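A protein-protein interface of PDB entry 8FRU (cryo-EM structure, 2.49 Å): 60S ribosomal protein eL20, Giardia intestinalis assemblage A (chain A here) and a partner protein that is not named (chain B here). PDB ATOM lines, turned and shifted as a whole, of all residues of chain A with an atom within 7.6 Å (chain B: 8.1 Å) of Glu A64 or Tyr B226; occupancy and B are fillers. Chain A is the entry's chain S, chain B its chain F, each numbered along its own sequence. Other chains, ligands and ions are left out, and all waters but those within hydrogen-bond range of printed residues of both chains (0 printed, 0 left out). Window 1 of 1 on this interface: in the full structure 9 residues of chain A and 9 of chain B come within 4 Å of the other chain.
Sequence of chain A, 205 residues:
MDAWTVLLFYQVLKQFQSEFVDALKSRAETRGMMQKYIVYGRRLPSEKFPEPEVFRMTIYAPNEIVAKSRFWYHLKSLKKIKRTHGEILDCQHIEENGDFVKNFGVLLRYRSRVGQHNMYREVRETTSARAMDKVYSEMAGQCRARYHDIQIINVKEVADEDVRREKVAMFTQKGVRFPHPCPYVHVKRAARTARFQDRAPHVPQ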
ATOM      1  N   GLN A  35      -1.091  32.178  23.791  1.00  0.00           N
ATOM      2  CA  GLN A  35      -0.628  31.299  22.736  1.00  0.00           C
ATOM      3  C   GLN A  35      -0.570  32.102  21.449  1.00  0.00           C
ATOM      4  O   GLN A  35      -1.064  33.227  21.379  1.00  0.00           O
ATOM      5  CB  GLN A  35      -1.552  30.092  22.574  1.00  0.00           C
ATOM      6  CG  GLN A  35      -1.100  28.855  23.304  1.00  0.00           C
ATOM      7  CD  GLN A  35      -1.579  28.819  24.724  1.00  0.00           C
ATOM      8  OE1 GLN A  35      -0.809  29.040  25.655  1.00  0.00           O
ATOM      9  NE2 GLN A  35      -2.862  28.543  24.905  1.00  0.00           N
ATOM     10  N   TYR A  37      -1.443  31.809  17.259  1.00  0.00           N
ATOM     11  CA  TYR A  37      -2.231  31.057  16.298  1.00  0.00           C
ATOM     12  C   TYR A  37      -2.060  31.653  14.912  1.00  0.00           C
ATOM     13  O   TYR A  37      -1.878  32.861  14.758  1.00  0.00           O
ATOM     14  CB  TYR A  37      -3.726  31.065  16.655  1.00  0.00           C
ATOM     15  CG  TYR A  37      -4.071  30.418  17.969  1.00  0.00           C
ATOM     16  CD1 TYR A  37      -3.989  31.126  19.155  1.00  0.00           C
ATOM     17  CD2 TYR A  37      -4.497  29.105  18.021  1.00  0.00           C
ATOM     18  CE1 TYR A  37      -4.304  30.540  20.352  1.00  0.00           C
ATOM     19  CE2 TYR A  37      -4.815  28.513  19.211  1.00  0.00           C
ATOM     20  CZ  TYR A  37      -4.716  29.232  20.374  1.00  0.00           C
ATOM     21  OH  TYR A  37      -5.036  28.638  21.568  1.00  0.00           O
ATOM     22  N   VAL A  39      -4.395  31.823  11.561  1.00  0.00           N
ATOM     23  CA  VAL A  39      -5.783  31.626  11.168  1.00  0.00           C
ATOM     24  C   VAL A  39      -5.921  31.941   9.688  1.00  0.00           C
ATOM     25  O   VAL A  39      -5.402  32.954   9.212  1.00  0.00           O
ATOM     26  CB  VAL A  39      -6.740  32.495  12.001  1.00  0.00           C
ATOM     27  CG1 VAL A  39      -8.173  32.141  11.685  1.00  0.00           C
ATOM     28  CG2 VAL A  39      -6.461  32.320  13.476  1.00  0.00           C
ATOM     29  N   ILE A  59      -2.306  35.632  15.403  1.00  0.00           N
ATOM     30  CA  ILE A  59      -3.075  36.083  16.554  1.00  0.00           C
ATOM     31  C   ILE A  59      -2.461  35.518  17.823  1.00  0.00           C
ATOM     32  O   ILE A  59      -2.044  34.358  17.861  1.00  0.00           O
ATOM     33  CB  ILE A  59      -4.559  35.665  16.446  1.00  0.00           C
ATOM     34  CG1 ILE A  59      -5.126  36.030  15.076  1.00  0.00           C
ATOM     35  CG2 ILE A  59      -5.372  36.314  17.542  1.00  0.00           C
ATOM     36  CD1 ILE A  59      -5.646  37.427  14.985  1.00  0.00           C
ATOM     37  N   ALA A  61      -3.599  34.858  21.738  1.00  0.00           N
ATOM     38  CA  ALA A  61      -4.835  34.778  22.501  1.00  0.00           C
ATOM     39  C   ALA A  61      -4.689  33.699  23.558  1.00  0.00           C
ATOM     40  O   ALA A  61      -3.782  32.866  23.479  1.00  0.00           O
ATOM     41  CB  ALA A  61      -6.034  34.486  21.590  1.00  0.00           C
ATOM     42  N   PRO A  62      -5.560  33.697  24.572  1.00  0.00           N
ATOM     43  CA  PRO A  62      -5.529  32.617  25.568  1.00  0.00           C
ATOM     44  C   PRO A  62      -6.147  31.303  25.111  1.00  0.00           C
ATOM     45  O   PRO A  62      -5.785  30.257  25.662  1.00  0.00           O
ATOM     46  CB  PRO A  62      -6.303  33.215  26.746  1.00  0.00           C
ATOM     47  CG  PRO A  62      -7.190  34.204  26.131  1.00  0.00           C
ATOM     48  CD  PRO A  62      -6.419  34.808  25.004  1.00  0.00           C
ATOM     49  N   ASN A  63      -7.058  31.304  24.141  1.00  0.00           N
ATOM     50  CA  ASN A  63      -7.542  30.062  23.551  1.00  0.00           C
ATOM     51  C   ASN A  63      -8.034  30.352  22.139  1.00  0.00           C
ATOM     52  O   ASN A  63      -7.998  31.491  21.670  1.00  0.00           O
ATOM     53  CB  ASN A  63      -8.632  29.402  24.408  1.00  0.00           C
ATOM     54  CG  ASN A  63      -9.766  30.342  24.756  1.00  0.00           C
ATOM     55  OD1 ASN A  63     -10.716  30.484  23.998  1.00  0.00           O
ATOM     56  ND2 ASN A  63      -9.683  30.968  25.920  1.00  0.00           N
ATOM     57  N   GLU A  64      -8.494  29.301  21.455  1.00  0.00           N
ATOM     58  CA  GLU A  64      -8.817  29.415  20.038  1.00  0.00           C
ATOM     59  C   GLU A  64     -10.150  30.111  19.783  1.00  0.00           C
ATOM     60  O   GLU A  64     -10.331  30.712  18.717  1.00  0.00           O
ATOM     61  CB  GLU A  64      -8.806  28.032  19.393  1.00  0.00           C
ATOM     62  CG  GLU A  64      -9.899  27.114  19.866  1.00  0.00           C
ATOM     63  CD  GLU A  64     -10.342  26.151  18.788  1.00  0.00           C
ATOM     64  OE1 GLU A  64      -9.551  25.899  17.857  1.00  0.00           O
ATOM     65  OE2 GLU A  64     -11.483  25.646  18.870  1.00  0.00           O
ATOM     66  N   ILE A  65     -11.085  30.053  20.731  1.00  0.00           N
ATOM     67  CA  ILE A  65     -12.333  30.801  20.590  1.00  0.00           C
ATOM     68  C   ILE A  65     -12.040  32.294  20.499  1.00  0.00           C
ATOM     69  O   ILE A  65     -12.539  33.000  19.610  1.00  0.00           O
ATOM     70  CB  ILE A  65     -13.277  30.484  21.764  1.00  0.00           C
ATOM     71  CG1 ILE A  65     -13.384  28.974  21.991  1.00  0.00           C
ATOM     72  CG2 ILE A  65     -14.654  31.074  21.526  1.00  0.00           C
ATOM     73  CD1 ILE A  65     -14.424  28.294  21.152  1.00  0.00           C
ATOM     74  N   VAL A  66     -11.201  32.789  21.409  1.00  0.00           N
ATOM     75  CA  VAL A  66     -10.799  34.191  21.388  1.00  0.00           C
ATOM     76  C   VAL A  66     -10.038  34.504  20.109  1.00  0.00           C
ATOM     77  O   VAL A  66     -10.162  35.597  19.541  1.00  0.00           O
ATOM     78  CB  VAL A  66      -9.960  34.516  22.637  1.00  0.00           C
ATOM     79  CG1 VAL A  66      -9.531  35.967  22.627  1.00  0.00           C
ATOM     80  CG2 VAL A  66     -10.726  34.178  23.897  1.00  0.00           C
ATOM     81  N   ALA A  67      -9.223  33.558  19.647  1.00  0.00           N
ATOM     82  CA  ALA A  67      -8.450  33.771  18.432  1.00  0.00           C
ATOM     83  C   ALA A  67      -9.361  34.004  17.238  1.00  0.00           C
ATOM     84  O   ALA A  67      -9.153  34.936  16.456  1.00  0.00           O
ATOM     85  CB  ALA A  67      -7.531  32.577  18.186  1.00  0.00           C
ATOM     86  N   LYS A  68     -10.381  33.163  17.082  1.00  0.00           N
ATOM     87  CA  LYS A  68     -11.306  33.343  15.969  1.00  0.00           C
ATOM     88  C   LYS A  68     -12.109  34.629  16.117  1.00  0.00           C
ATOM     89  O   LYS A  68     -12.384  35.314  15.124  1.00  0.00           O
ATOM     90  CB  LYS A  68     -12.225  32.135  15.857  1.00  0.00           C
ATOM     91  CG  LYS A  68     -11.481  30.858  15.585  1.00  0.00           C
ATOM     92  CD  LYS A  68     -12.387  29.653  15.670  1.00  0.00           C
ATOM     93  CE  LYS A  68     -11.583  28.375  15.582  1.00  0.00           C
ATOM     94  NZ  LYS A  68     -12.444  27.168  15.626  1.00  0.00           N
ATOM     95  N   SER A  69     -12.491  34.979  17.345  1.00  0.00           N
ATOM     96  CA  SER A  69     -13.195  36.241  17.545  1.00  0.00           C
ATOM     97  C   SER A  69     -12.359  37.418  17.060  1.00  0.00           C
ATOM     98  O   SER A  69     -12.859  38.296  16.349  1.00  0.00           O
ATOM     99  CB  SER A  69     -13.560  36.416  19.016  1.00  0.00           C
ATOM    100  OG  SER A  69     -14.222  35.272  19.505  1.00  0.00           O
ATOM    101  N   ARG A  70     -11.079  37.451  17.430  1.00  0.00           N
ATOM    102  CA  ARG A  70     -10.221  38.558  17.014  1.00  0.00           C
ATOM    103  C   ARG A  70      -9.963  38.537  15.513  1.00  0.00           C
ATOM    104  O   ARG A  70      -9.871  39.595  14.875  1.00  0.00           O
ATOM    105  CB  ARG A  70      -8.907  38.521  17.784  1.00  0.00           C
ATOM    106  CG  ARG A  70      -9.030  38.974  19.220  1.00  0.00           C
ATOM    107  CD  ARG A  70      -8.691  40.443  19.365  1.00  0.00           C
ATOM    108  NE  ARG A  70      -9.879  41.252  19.595  1.00  0.00           N
ATOM    109  CZ  ARG A  70      -9.873  42.570  19.738  1.00  0.00           C
ATOM    110  NH1 ARG A  70      -8.751  43.265  19.681  1.00  0.00           N
ATOM    111  NH2 ARG A  70     -11.023  43.205  19.941  1.00  0.00           N
ATOM    112  N   ILE A  88     -14.030  30.203   8.302  1.00  0.00           N
ATOM    113  CA  ILE A  88     -12.665  30.022   8.776  1.00  0.00           C
ATOM    114  C   ILE A  88     -12.171  28.662   8.316  1.00  0.00           C
ATOM    115  O   ILE A  88     -12.799  27.635   8.593  1.00  0.00           O
ATOM    116  CB  ILE A  88     -12.578  30.154  10.304  1.00  0.00           C
ATOM    117  CG1 ILE A  88     -12.492  31.625  10.697  1.00  0.00           C
ATOM    118  CG2 ILE A  88     -11.390  29.378  10.839  1.00  0.00           C
ATOM    119  CD1 ILE A  88     -12.397  31.839  12.168  1.00  0.00           C
ATOM    120  N   ASP A  90      -8.947  27.278   8.877  1.00  0.00           N
ATOM    121  CA  ASP A  90      -8.044  26.541   9.748  1.00  0.00           C
ATOM    122  C   ASP A  90      -7.447  27.445  10.818  1.00  0.00           C
ATOM    123  O   ASP A  90      -7.003  28.557  10.524  1.00  0.00           O
ATOM    124  CB  ASP A  90      -6.935  25.893   8.917  1.00  0.00           C
ATOM    125  CG  ASP A  90      -5.715  25.550   9.733  1.00  0.00           C
ATOM    126  OD1 ASP A  90      -5.871  25.203  10.919  1.00  0.00           O
ATOM    127  OD2 ASP A  90      -4.593  25.633   9.192  1.00  0.00           O
ATOM    128  N   CYS A  91      -7.428  26.967  12.057  1.00  0.00           N
ATOM    129  CA  CYS A  91      -6.855  27.671  13.204  1.00  0.00           C
ATOM    130  C   CYS A  91      -5.807  26.745  13.809  1.00  0.00           C
ATOM    131  O   CYS A  91      -6.146  25.841  14.578  1.00  0.00           O
ATOM    132  CB  CYS A  91      -7.942  28.026  14.216  1.00  0.00           C
ATOM    133  SG  CYS A  91      -7.486  29.220  15.492  1.00  0.00           S
ATOM    134  N   GLN A  92      -4.541  26.955  13.472  1.00  0.00           N
ATOM    135  CA  GLN A  92      -3.475  26.033  13.844  1.00  0.00           C
ATOM    136  C   GLN A  92      -2.612  26.637  14.941  1.00  0.00           C
ATOM    137  O   GLN A  92      -2.047  27.720  14.768  1.00  0.00           O
ATOM    138  CB  GLN A  92      -2.625  25.666  12.629  1.00  0.00           C
ATOM    139  CG  GLN A  92      -2.549  26.737  11.566  1.00  0.00           C
ATOM    140  CD  GLN A  92      -1.592  26.372  10.446  1.00  0.00           C
ATOM    141  OE1 GLN A  92      -0.498  26.923  10.346  1.00  0.00           O
ATOM    142  NE2 GLN A  92      -2.001  25.435   9.599  1.00  0.00           N
ATOM    143  N   HIS A  93      -2.508  25.927  16.062  1.00  0.00           N
ATOM    144  CA  HIS A  93      -1.649  26.333  17.164  1.00  0.00           C
ATOM    145  C   HIS A  93      -0.195  26.014  16.853  1.00  0.00           C
ATOM    146  O   HIS A  93       0.126  24.931  16.358  1.00  0.00           O
ATOM    147  CB  HIS A  93      -2.075  25.625  18.449  1.00  0.00           C
ATOM    148  CG  HIS A  93      -1.220  25.949  19.631  1.00  0.00           C
ATOM    149  ND1 HIS A  93      -0.320  25.052  20.165  1.00  0.00           N
ATOM    150  CD2 HIS A  93      -1.127  27.068  20.386  1.00  0.00           C
ATOM    151  CE1 HIS A  93       0.292  25.606  21.195  1.00  0.00           C
ATOM    152  NE2 HIS A  93      -0.179  26.829  21.350  1.00  0.00           N
ATOM    153  N   THR B 130     -24.948  28.065  27.749  1.00  0.00           N
ATOM    154  CA  THR B 130     -23.641  27.847  27.153  1.00  0.00           C
ATOM    155  C   THR B 130     -23.702  26.522  26.410  1.00  0.00           C
ATOM    156  O   THR B 130     -24.397  25.602  26.843  1.00  0.00           O
ATOM    157  CB  THR B 130     -22.522  27.860  28.212  1.00  0.00           C
ATOM    158  OG1 THR B 130     -21.270  28.142  27.583  1.00  0.00           O
ATOM    159  CG2 THR B 130     -22.428  26.538  28.942  1.00  0.00           C
ATOM    160  N   TYR B 131     -23.005  26.432  25.279  1.00  0.00           N
ATOM    161  CA  TYR B 131     -23.162  25.284  24.397  1.00  0.00           C
ATOM    162  C   TYR B 131     -21.874  25.016  23.634  1.00  0.00           C
ATOM    163  O   TYR B 131     -20.945  25.823  23.632  1.00  0.00           O
ATOM    164  CB  TYR B 131     -24.321  25.486  23.422  1.00  0.00           C
ATOM    165  CG  TYR B 131     -24.264  26.784  22.672  1.00  0.00           C
ATOM    166  CD1 TYR B 131     -24.793  27.938  23.214  1.00  0.00           C
ATOM    167  CD2 TYR B 131     -23.681  26.857  21.423  1.00  0.00           C
ATOM    168  CE1 TYR B 131     -24.744  29.122  22.537  1.00  0.00           C
ATOM    169  CE2 TYR B 131     -23.628  28.036  20.738  1.00  0.00           C
ATOM    170  CZ  TYR B 131     -24.163  29.168  21.298  1.00  0.00           C
ATOM    171  OH  TYR B 131     -24.112  30.355  20.615  1.00  0.00           O
ATOM    172  N   GLY B 132     -21.838  23.861  22.982  1.00  0.00           N
ATOM    173  CA  GLY B 132     -20.670  23.449  22.231  1.00  0.00           C
ATOM    174  C   GLY B 132     -20.884  22.085  21.615  1.00  0.00           C
ATOM    175  O   GLY B 132     -21.983  21.541  21.640  1.00  0.00           O
ATOM    176  N   GLU B 133     -19.804  21.534  21.062  1.00  0.00           N
ATOM    177  CA  GLU B 133     -19.849  20.249  20.371  1.00  0.00           C
ATOM    178  C   GLU B 133     -19.316  19.147  21.267  1.00  0.00           C
ATOM    179  O   GLU B 133     -18.162  19.228  21.706  1.00  0.00           O
ATOM    180  CB  GLU B 133     -19.037  20.311  19.087  1.00  0.00           C
ATOM    181  CG  GLU B 133     -19.155  21.632  18.362  1.00  0.00           C
ATOM    182  CD  GLU B 133     -17.985  22.547  18.627  1.00  0.00           C
ATOM    183  OE1 GLU B 133     -16.884  22.034  18.910  1.00  0.00           O
ATOM    184  OE2 GLU B 133     -18.163  23.779  18.547  1.00  0.00           O
ATOM    185  N   PRO B 134     -20.094  18.109  21.556  1.00  0.00           N
ATOM    186  CA  PRO B 134     -19.647  17.060  22.473  1.00  0.00           C
ATOM    187  C   PRO B 134     -18.892  15.931  21.782  1.00  0.00           C
ATOM    188  O   PRO B 134     -18.933  15.762  20.564  1.00  0.00           O
ATOM    189  CB  PRO B 134     -20.969  16.543  23.051  1.00  0.00           C
ATOM    190  CG  PRO B 134     -21.944  16.730  21.940  1.00  0.00           C
ATOM    191  CD  PRO B 134     -21.479  17.893  21.106  1.00  0.00           C
ATOM    192  N   PHE B 214     -18.231  34.079  26.918  1.00  0.00           N
ATOM    193  CA  PHE B 214     -17.001  33.298  27.015  1.00  0.00           C
ATOM    194  C   PHE B 214     -15.871  33.925  26.208  1.00  0.00           C
ATOM    195  O   PHE B 214     -14.699  33.789  26.573  1.00  0.00           O
ATOM    196  CB  PHE B 214     -17.264  31.866  26.545  1.00  0.00           C
ATOM    197  CG  PHE B 214     -16.105  30.931  26.736  1.00  0.00           C
ATOM    198  CD1 PHE B 214     -15.919  30.277  27.934  1.00  0.00           C
ATOM    199  CD2 PHE B 214     -15.202  30.703  25.714  1.00  0.00           C
ATOM    200  CE1 PHE B 214     -14.862  29.420  28.108  1.00  0.00           C
ATOM    201  CE2 PHE B 214     -14.144  29.847  25.887  1.00  0.00           C
ATOM    202  CZ  PHE B 214     -13.974  29.205  27.085  1.00  0.00           C
ATOM    203  N   TYR B 222     -20.961  30.531  23.222  1.00  0.00           N
ATOM    204  CA  TYR B 222     -20.353  29.419  22.506  1.00  0.00           C
ATOM    205  C   TYR B 222     -18.976  29.112  23.083  1.00  0.00           C
ATOM    206  O   TYR B 222     -18.120  29.996  23.158  1.00  0.00           O
ATOM    207  CB  TYR B 222     -20.260  29.758  21.020  1.00  0.00           C
ATOM    208  CG  TYR B 222     -19.538  28.733  20.197  1.00  0.00           C
ATOM    209  CD1 TYR B 222     -20.080  27.481  19.992  1.00  0.00           C
ATOM    210  CD2 TYR B 222     -18.314  29.017  19.624  1.00  0.00           C
ATOM    211  CE1 TYR B 222     -19.427  26.545  19.244  1.00  0.00           C
ATOM    212  CE2 TYR B 222     -17.654  28.085  18.876  1.00  0.00           C
ATOM    213  CZ  TYR B 222     -18.216  26.850  18.688  1.00  0.00           C
ATOM    214  OH  TYR B 222     -17.565  25.905  17.939  1.00  0.00           O
ATOM    215  N   ARG B 223     -18.763  27.858  23.479  1.00  0.00           N
ATOM    216  CA  ARG B 223     -17.492  27.413  24.034  1.00  0.00           C
ATOM    217  C   ARG B 223     -16.737  26.454  23.135  1.00  0.00           C
ATOM    218  O   ARG B 223     -15.594  26.117  23.454  1.00  0.00           O
ATOM    219  CB  ARG B 223     -17.697  26.716  25.386  1.00  0.00           C
ATOM    220  CG  ARG B 223     -18.140  27.594  26.506  1.00  0.00           C
ATOM    221  CD  ARG B 223     -18.641  26.757  27.649  1.00  0.00           C
ATOM    222  NE  ARG B 223     -17.700  26.730  28.757  1.00  0.00           N
ATOM    223  CZ  ARG B 223     -17.776  27.507  29.826  1.00  0.00           C
ATOM    224  NH1 ARG B 223     -18.752  28.384  29.975  1.00  0.00           N
ATOM    225  NH2 ARG B 223     -16.848  27.401  30.767  1.00  0.00           N
ATOM    226  N   GLY B 224     -17.339  25.978  22.057  1.00  0.00           N
ATOM    227  CA  GLY B 224     -16.666  24.982  21.241  1.00  0.00           C
ATOM    228  C   GLY B 224     -16.499  23.678  21.994  1.00  0.00           C
ATOM    229  O   GLY B 224     -17.460  23.116  22.525  1.00  0.00           O
ATOM    230  N   LYS B 225     -15.266  23.182  22.047  1.00  0.00           N
ATOM    231  CA  LYS B 225     -14.972  21.886  22.643  1.00  0.00           C
ATOM    232  C   LYS B 225     -14.770  21.934  24.150  1.00  0.00           C
ATOM    233  O   LYS B 225     -14.712  20.877  24.782  1.00  0.00           O
ATOM    234  CB  LYS B 225     -13.725  21.285  21.996  1.00  0.00           C
ATOM    235  CG  LYS B 225     -12.609  22.280  21.799  1.00  0.00           C
ATOM    236  CD  LYS B 225     -11.253  21.627  21.954  1.00  0.00           C
ATOM    237  CE  LYS B 225     -11.098  21.006  23.330  1.00  0.00           C
ATOM    238  NZ  LYS B 225     -11.309  22.004  24.409  1.00  0.00           N
ATOM    239  N   TYR B 226     -14.656  23.118  24.744  1.00  0.00           N
ATOM    240  CA  TYR B 226     -14.485  23.201  26.185  1.00  0.00           C
ATOM    241  C   TYR B 226     -15.752  22.836  26.941  1.00  0.00           C
ATOM    242  O   TYR B 226     -15.699  22.648  28.165  1.00  0.00           O
ATOM    243  CB  TYR B 226     -14.014  24.602  26.557  1.00  0.00           C
ATOM    244  CG  TYR B 226     -12.782  25.017  25.796  1.00  0.00           C
ATOM    245  CD1 TYR B 226     -11.526  24.582  26.181  1.00  0.00           C
ATOM    246  CD2 TYR B 226     -12.877  25.829  24.682  1.00  0.00           C
ATOM    247  CE1 TYR B 226     -10.399  24.955  25.482  1.00  0.00           C
ATOM    248  CE2 TYR B 226     -11.758  26.205  23.975  1.00  0.00           C
ATOM    249  CZ  TYR B 226     -10.522  25.767  24.378  1.00  0.00           C
ATOM    250  OH  TYR B 226      -9.407  26.144  23.672  1.00  0.00           O
ATOM    251  N   ILE B 227     -16.878  22.720  26.235  1.00  0.00           N
ATOM    252  CA  ILE B 227     -18.104  22.217  26.841  1.00  0.00           C
ATOM    253  C   ILE B 227     -17.864  20.845  27.445  1.00  0.00           C
ATOM    254  O   ILE B 227     -18.489  20.478  28.444  1.00  0.00           O
ATOM    255  CB  ILE B 227     -19.235  22.190  25.792  1.00  0.00           C
ATOM    256  CG1 ILE B 227     -20.606  22.063  26.460  1.00  0.00           C
ATOM    257  CG2 ILE B 227     -19.023  21.055  24.816  1.00  0.00           C
ATOM    258  CD1 ILE B 227     -21.135  23.348  27.021  1.00  0.00           C
ATOM    259  N   ASN B 228     -16.928  20.085  26.879  1.00  0.00           N
ATOM    260  CA  ASN B 228     -16.688  18.726  27.346  1.00  0.00           C
ATOM    261  C   ASN B 228     -16.148  18.709  28.769  1.00  0.00           C
ATOM    262  O   ASN B 228     -16.660  17.984  29.624  1.00  0.00           O
ATOM    263  CB  ASN B 228     -15.746  18.011  26.385  1.00  0.00           C
ATOM    264  CG  ASN B 228     -16.419  17.665  25.081  1.00  0.00           C
ATOM    265  OD1 ASN B 228     -17.376  16.900  25.054  1.00  0.00           O
ATOM    266  ND2 ASN B 228     -15.933  18.235  23.995  1.00  0.00           N
ATOM    267  N   GLU B 229     -15.126  19.514  29.054  1.00  0.00           N
ATOM    268  CA  GLU B 229     -14.636  19.594  30.428  1.00  0.00           C
ATOM    269  C   GLU B 229     -15.644  20.291  31.336  1.00  0.00           C
ATOM    270  O   GLU B 229     -15.923  19.819  32.456  1.00  0.00           O
ATOM    271  CB  GLU B 229     -13.288  20.310  30.459  1.00  0.00           C
ATOM    272  CG  GLU B 229     -13.168  21.441  29.462  1.00  0.00           C
ATOM    273  CD  GLU B 229     -12.427  21.039  28.193  1.00  0.00           C
ATOM    274  OE1 GLU B 229     -12.865  20.089  27.509  1.00  0.00           O
ATOM    275  OE2 GLU B 229     -11.402  21.676  27.876  1.00  0.00           O
ATOM    276  N   PHE B 230     -16.226  21.396  30.854  1.00  0.00           N
ATOM    277  CA  PHE B 230     -17.212  22.120  31.645  1.00  0.00           C
ATOM    278  C   PHE B 230     -18.294  21.187  32.160  1.00  0.00           C
ATOM    279  O   PHE B 230     -18.748  21.319  33.299  1.00  0.00           O
ATOM    280  CB  PHE B 230     -17.832  23.238  30.809  1.00  0.00           C
ATOM    281  CG  PHE B 230     -18.930  23.979  31.507  1.00  0.00           C
ATOM    282  CD1 PHE B 230     -18.644  25.030  32.352  1.00  0.00           C
ATOM    283  CD2 PHE B 230     -20.249  23.621  31.323  1.00  0.00           C
ATOM    284  CE1 PHE B 230     -19.652  25.707  32.994  1.00  0.00           C
ATOM    285  CE2 PHE B 230     -21.256  24.290  31.967  1.00  0.00           C
ATOM    286  CZ  PHE B 230     -20.959  25.334  32.801  1.00  0.00           C
ATOM    287  N   VAL B 231     -18.717  20.233  31.335  1.00  0.00           N
ATOM    288  CA  VAL B 231     -19.766  19.312  31.741  1.00  0.00           C
ATOM    289  C   VAL B 231     -19.208  18.110  32.496  1.00  0.00           C
ATOM    290  O   VAL B 231     -19.860  17.606  33.413  1.00  0.00           O
ATOM    291  CB  VAL B 231     -20.575  18.871  30.510  1.00  0.00           C
ATOM    292  CG1 VAL B 231     -20.497  17.371  30.321  1.00  0.00           C
ATOM    293  CG2 VAL B 231     -22.006  19.336  30.625  1.00  0.00           C
ATOM    294  N   ALA B 232     -18.012  17.636  32.139  1.00  0.00           N
ATOM    295  CA  ALA B 232     -17.423  16.511  32.851  1.00  0.00           C
ATOM    296  C   ALA B 232     -17.338  16.788  34.337  1.00  0.00           C
ATOM    297  O   ALA B 232     -17.473  15.869  35.152  1.00  0.00           O
ATOM    298  CB  ALA B 232     -16.036  16.204  32.295  1.00  0.00           C
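The side-chain carboxylate of Glu A64 is in salt-bridge range of the side-chain amino group of Lys A68, at 3.7 Å.
The side-chain amide oxygen of Asn A63 is in hydrogen-bond range of the backbone NH of Ile A65 (3.3 Å).
The backbone carbonyl oxygen of Ile A65 lies within hydrogen-bond range of the side-chain hydroxyl of Ser A69, at 2.8 Å.
The backbone carbonyl oxygen (O) of Gly B224 lies within hydrogen-bond range of the backbone NH (N) of Glu B133, at 3.2 Å.
The guanidinium group (NH1) of Arg B223 sits close to the side-chain hydroxyl (OG1) of Thr B130, 3.5 Å away.
O of Tyr B131 sits at hydrogen-bond distance from N of Arg B223 (3.0 Å).
Among the printed residues, merely in contact across the chains: Asn A63 with Phe B214 (3.97 Å), Asn A63 with Tyr B226 (3.4 Å), Glu A64 with Tyr B226 (3.96 Å), Ile A65 with Tyr B222 (3.96 Å), Ile A65 with Arg B223 (3.4 Å), Ile A65 with Gly B224 (3.8 Å) and Ile A65 with Tyr B226 (3.8 Å).
Printed residues of chain A within 4 Å of Phe B214: Asn A63.
Of the printed residues of chain B, Ile A65 touches Tyr B222 (3.96 Å), Arg B223 (3.4 Å), Gly B224 (3.8 Å) and Tyr B226 (3.8 Å).
Tyr A37 touches none of the printed residues of chain B.
The nearest residue of chain B that does not touch Glu A64 is Lys B225 (4.6 Å).
The nearest residue of chain A that does not touch Tyr B226 is Tyr A37 (5.5 Å).
The nearest printed residue of chain A that does not touch Phe B214 is Ile A65 (4.1 Å).
Of the 19 printed residues of chain A, 3 touch a printed residue of chain B.
Of the 17 printed residues of chain B, 5 touch a printed residue of chain A.
Hydrophobic or aromatic side chains of chain B within 4 Å of the printed part of chain A: Phe B214, Tyr B222 and Tyr B226.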
